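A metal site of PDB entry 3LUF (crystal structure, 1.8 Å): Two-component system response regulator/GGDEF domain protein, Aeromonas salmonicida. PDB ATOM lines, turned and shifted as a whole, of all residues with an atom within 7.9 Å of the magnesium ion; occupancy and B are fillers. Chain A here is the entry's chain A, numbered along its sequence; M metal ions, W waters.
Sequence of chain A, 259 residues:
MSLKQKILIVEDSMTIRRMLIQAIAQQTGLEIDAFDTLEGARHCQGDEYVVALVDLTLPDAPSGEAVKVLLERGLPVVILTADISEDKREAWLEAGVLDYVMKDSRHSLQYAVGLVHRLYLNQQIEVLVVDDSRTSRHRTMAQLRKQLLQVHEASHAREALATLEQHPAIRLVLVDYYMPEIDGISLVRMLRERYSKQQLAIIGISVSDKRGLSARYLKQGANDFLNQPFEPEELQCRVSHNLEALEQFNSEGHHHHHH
Glu 11 touches the magnesium ion.
Water W1 lies within hydrogen-bond range of the side-chain carboxylate of Glu 11 (2.7 Å) and the side-chain amino group of Lys 103 (2.9 Å).
NZ of Lys 103 lies within salt-bridge range of OD1 of Asp 55, 2.9 Å away.
O of Val 10 is in hydrogen-bond range of N of Asp 55, at 2.8 Å.
The side-chain carboxylate of Glu 11 is in salt-bridge range of the side-chain amino group of Lys 103, 2.8 Å away.
OE2 of Glu 11 lies within hydrogen-bond range of N of Ser 13 (2.8 Å).
The magnesium ion is bound by the side-chain hydroxyl (OG1) of Thr 57 (2.0 Å), water W1 (2.0 Å), the backbone carbonyl oxygen (O) of Thr 57 (2.1 Å), the side-chain carboxylate (OD2) of Asp 12 (2.1 Å), the side-chain carboxylate (OD2) of Asp 55 (2.1 Å) and water W2 (2.1 Å).
The magnesium ion has six donor atoms within binding distance.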
ATOM      1  N   VAL A  10     -25.700 -20.882   3.138  1.00  0.00           N
ATOM      2  CA  VAL A  10     -26.757 -20.410   4.023  1.00  0.00           C
ATOM      3  C   VAL A  10     -26.873 -21.403   5.179  1.00  0.00           C
ATOM      4  O   VAL A  10     -27.381 -22.514   5.018  1.00  0.00           O
ATOM      5  CB  VAL A  10     -28.100 -20.235   3.261  1.00  0.00           C
ATOM      6  CG1 VAL A  10     -29.070 -19.426   4.122  1.00  0.00           C
ATOM      7  CG2 VAL A  10     -27.865 -19.484   1.929  1.00  0.00           C
ATOM      8  N   GLU A  11     -26.372 -20.996   6.343  1.00  0.00           N
ATOM      9  CA  GLU A  11     -26.167 -21.930   7.469  1.00  0.00           C
ATOM     10  C   GLU A  11     -26.085 -21.086   8.744  1.00  0.00           C
ATOM     11  O   GLU A  11     -25.251 -20.171   8.824  1.00  0.00           O
ATOM     12  CB  GLU A  11     -24.817 -22.668   7.250  1.00  0.00           C
ATOM     13  CG  GLU A  11     -24.275 -23.457   8.515  1.00  0.00           C
ATOM     14  CD  GLU A  11     -25.229 -24.514   9.010  1.00  0.00           C
ATOM     15  OE1 GLU A  11     -25.373 -25.585   8.342  1.00  0.00           O
ATOM     16  OE2 GLU A  11     -25.810 -24.309  10.122  1.00  0.00           O
ATOM     17  N   ASP A  12     -26.953 -21.367   9.702  1.00  0.00           N
ATOM     18  CA  ASP A  12     -26.961 -20.538  10.908  1.00  0.00           C
ATOM     19  C   ASP A  12     -25.925 -20.913  11.957  1.00  0.00           C
ATOM     20  O   ASP A  12     -25.598 -20.087  12.794  1.00  0.00           O
ATOM     21  CB  ASP A  12     -28.349 -20.426  11.551  1.00  0.00           C
ATOM     22  CG  ASP A  12     -28.943 -21.762  11.902  1.00  0.00           C
ATOM     23  OD1 ASP A  12     -29.696 -21.797  12.910  1.00  0.00           O
ATOM     24  OD2 ASP A  12     -28.765 -22.781  11.182  1.00  0.00           O
ATOM     25  N   SER A  13     -25.398 -22.131  11.912  1.00  0.00           N
ATOM     26  CA  SER A  13     -24.356 -22.496  12.871  1.00  0.00           C
ATOM     27  C   SER A  13     -23.111 -21.670  12.600  1.00  0.00           C
ATOM     28  O   SER A  13     -22.523 -21.747  11.531  1.00  0.00           O
ATOM     29  CB  SER A  13     -24.024 -23.994  12.795  1.00  0.00           C
ATOM     30  OG  SER A  13     -22.787 -24.229  13.485  1.00  0.00           O
ATOM     31  N   ILE A  16     -20.120 -24.198  11.921  1.00  0.00           N
ATOM     32  CA  ILE A  16     -20.120 -24.837  10.603  1.00  0.00           C
ATOM     33  C   ILE A  16     -19.861 -23.846   9.489  1.00  0.00           C
ATOM     34  O   ILE A  16     -19.104 -24.103   8.572  1.00  0.00           O
ATOM     35  CB  ILE A  16     -21.420 -25.623  10.368  1.00  0.00           C
ATOM     36  CG1 ILE A  16     -21.447 -26.795  11.369  1.00  0.00           C
ATOM     37  CG2 ILE A  16     -21.475 -26.198   8.931  1.00  0.00           C
ATOM     38  CD1 ILE A  16     -22.799 -27.367  11.568  1.00  0.00           C
ATOM     39  N   ASP A  36     -26.520 -16.294   7.754  1.00  0.00           N
ATOM     40  CA  ASP A  36     -27.153 -17.110   8.778  1.00  0.00           C
ATOM     41  C   ASP A  36     -28.680 -17.281   8.665  1.00  0.00           C
ATOM     42  O   ASP A  36     -29.250 -17.961   9.474  1.00  0.00           O
ATOM     43  CB  ASP A  36     -26.723 -16.671  10.208  1.00  0.00           C
ATOM     44  CG  ASP A  36     -27.053 -15.213  10.542  1.00  0.00           C
ATOM     45  OD1 ASP A  36     -27.724 -14.530   9.750  1.00  0.00           O
ATOM     46  OD2 ASP A  36     -26.638 -14.743  11.650  1.00  0.00           O
ATOM     47  N   ASP A  55     -28.353 -25.111   4.475  1.00  0.00           N
ATOM     48  CA  ASP A  55     -28.808 -25.776   5.700  1.00  0.00           C
ATOM     49  C   ASP A  55     -30.348 -25.947   5.683  1.00  0.00           C
ATOM     50  O   ASP A  55     -31.089 -25.029   5.254  1.00  0.00           O
ATOM     51  CB  ASP A  55     -28.395 -24.928   6.890  1.00  0.00           C
ATOM     52  CG  ASP A  55     -28.855 -25.494   8.223  1.00  0.00           C
ATOM     53  OD1 ASP A  55     -28.994 -26.723   8.381  1.00  0.00           O
ATOM     54  OD2 ASP A  55     -29.050 -24.678   9.112  1.00  0.00           O
ATOM     55  N   LEU A  56     -30.798 -27.110   6.144  1.00  0.00           N
ATOM     56  CA  LEU A  56     -32.246 -27.365   6.303  1.00  0.00           C
ATOM     57  C   LEU A  56     -32.822 -26.722   7.561  1.00  0.00           C
ATOM     58  O   LEU A  56     -34.044 -26.492   7.624  1.00  0.00           O
ATOM     59  CB  LEU A  56     -32.556 -28.863   6.282  1.00  0.00           C
ATOM     60  CG  LEU A  56     -31.928 -29.602   5.100  1.00  0.00           C
ATOM     61  CD1 LEU A  56     -32.258 -31.066   5.235  1.00  0.00           C
ATOM     62  CD2 LEU A  56     -32.418 -28.987   3.774  1.00  0.00           C
ATOM     63  N   THR A  57     -31.970 -26.431   8.564  1.00  0.00           N
ATOM     64  CA  THR A  57     -32.465 -25.851   9.840  1.00  0.00           C
ATOM     65  C   THR A  57     -32.181 -24.371   9.977  1.00  0.00           C
ATOM     66  O   THR A  57     -31.348 -23.959  10.769  1.00  0.00           O
ATOM     67  CB  THR A  57     -31.896 -26.574  11.053  1.00  0.00           C
ATOM     68  OG1 THR A  57     -30.458 -26.442  11.044  1.00  0.00           O
ATOM     69  CG2 THR A  57     -32.343 -28.048  11.034  1.00  0.00           C
ATOM     70  N   LEU A  58     -32.872 -23.542   9.198  1.00  0.00           N
ATOM     71  CA  LEU A  58     -32.566 -22.133   9.242  1.00  0.00           C
ATOM     72  C   LEU A  58     -33.618 -21.416  10.095  1.00  0.00           C
ATOM     73  O   LEU A  58     -34.759 -21.886  10.153  1.00  0.00           O
ATOM     74  CB  LEU A  58     -32.534 -21.509   7.818  1.00  0.00           C
ATOM     75  CG  LEU A  58     -31.377 -22.024   6.971  1.00  0.00           C
ATOM     76  CD1 LEU A  58     -31.612 -21.452   5.559  1.00  0.00           C
ATOM     77  CD2 LEU A  58     -30.019 -21.484   7.512  1.00  0.00           C
ATOM     78  N   PRO A  59     -33.235 -20.310  10.750  1.00  0.00           N
ATOM     79  CA  PRO A  59     -34.214 -19.698  11.669  1.00  0.00           C
ATOM     80  C   PRO A  59     -35.512 -19.249  10.960  1.00  0.00           C
ATOM     81  O   PRO A  59     -36.615 -19.338  11.535  1.00  0.00           O
ATOM     82  CB  PRO A  59     -33.464 -18.479  12.186  1.00  0.00           C
ATOM     83  CG  PRO A  59     -31.991 -18.717  11.928  1.00  0.00           C
ATOM     84  CD  PRO A  59     -31.921 -19.651  10.759  1.00  0.00           C
ATOM     85  N   ALA A  61     -36.360 -20.593   8.037  1.00  0.00           N
ATOM     86  CA  ALA A  61     -36.675 -21.728   7.170  1.00  0.00           C
ATOM     87  C   ALA A  61     -36.234 -23.000   7.854  1.00  0.00           C
ATOM     88  O   ALA A  61     -35.261 -23.620   7.449  1.00  0.00           O
ATOM     89  CB  ALA A  61     -35.965 -21.571   5.767  1.00  0.00           C
ATOM     90  N   PRO A  62     -36.921 -23.382   8.935  1.00  0.00           N
ATOM     91  CA  PRO A  62     -36.402 -24.464   9.806  1.00  0.00           C
ATOM     92  C   PRO A  62     -36.691 -25.893   9.339  1.00  0.00           C
ATOM     93  O   PRO A  62     -36.284 -26.883   9.998  1.00  0.00           O
ATOM     94  CB  PRO A  62     -37.109 -24.167  11.134  1.00  0.00           C
ATOM     95  CG  PRO A  62     -38.461 -23.501  10.698  1.00  0.00           C
ATOM     96  CD  PRO A  62     -38.189 -22.770   9.423  1.00  0.00           C
ATOM     97  N   LEU A  80     -26.928 -29.341   3.273  1.00  0.00           N
ATOM     98  CA  LEU A  80     -26.099 -29.683   4.412  1.00  0.00           C
ATOM     99  C   LEU A  80     -27.046 -30.340   5.403  1.00  0.00           C
ATOM    100  O   LEU A  80     -28.014 -29.721   5.845  1.00  0.00           O
ATOM    101  CB  LEU A  80     -25.525 -28.417   5.045  1.00  0.00           C
ATOM    102  CG  LEU A  80     -24.538 -27.610   4.202  1.00  0.00           C
ATOM    103  CD1 LEU A  80     -24.266 -26.246   4.841  1.00  0.00           C
ATOM    104  CD2 LEU A  80     -23.238 -28.368   3.982  1.00  0.00           C
ATOM    105  N   LYS A 103     -23.055 -33.115   7.762  1.00  0.00           N
ATOM    106  CA  LYS A 103     -22.335 -32.109   8.580  1.00  0.00           C
ATOM    107  C   LYS A 103     -22.205 -32.520  10.049  1.00  0.00           C
ATOM    108  O   LYS A 103     -22.083 -31.690  10.947  1.00  0.00           O
ATOM    109  CB  LYS A 103     -22.882 -30.673   8.377  1.00  0.00           C
ATOM    110  CG  LYS A 103     -24.337 -30.498   8.619  1.00  0.00           C
ATOM    111  CD  LYS A 103     -24.664 -29.016   8.883  1.00  0.00           C
ATOM    112  CE  LYS A 103     -26.165 -28.893   9.040  1.00  0.00           C
ATOM    113  NZ  LYS A 103     -26.588 -27.679   9.772  1.00  0.00           N
HETATM  114 MG    MG M   1     -29.467 -24.740  11.152  1.00  0.00          MG
HETATM  115  O   HOH W   1     -27.711 -25.605  11.515  1.00  0.00           O
HETATM  116  O   HOH W   2     -29.799 -24.404  13.205  1.00  0.00           O
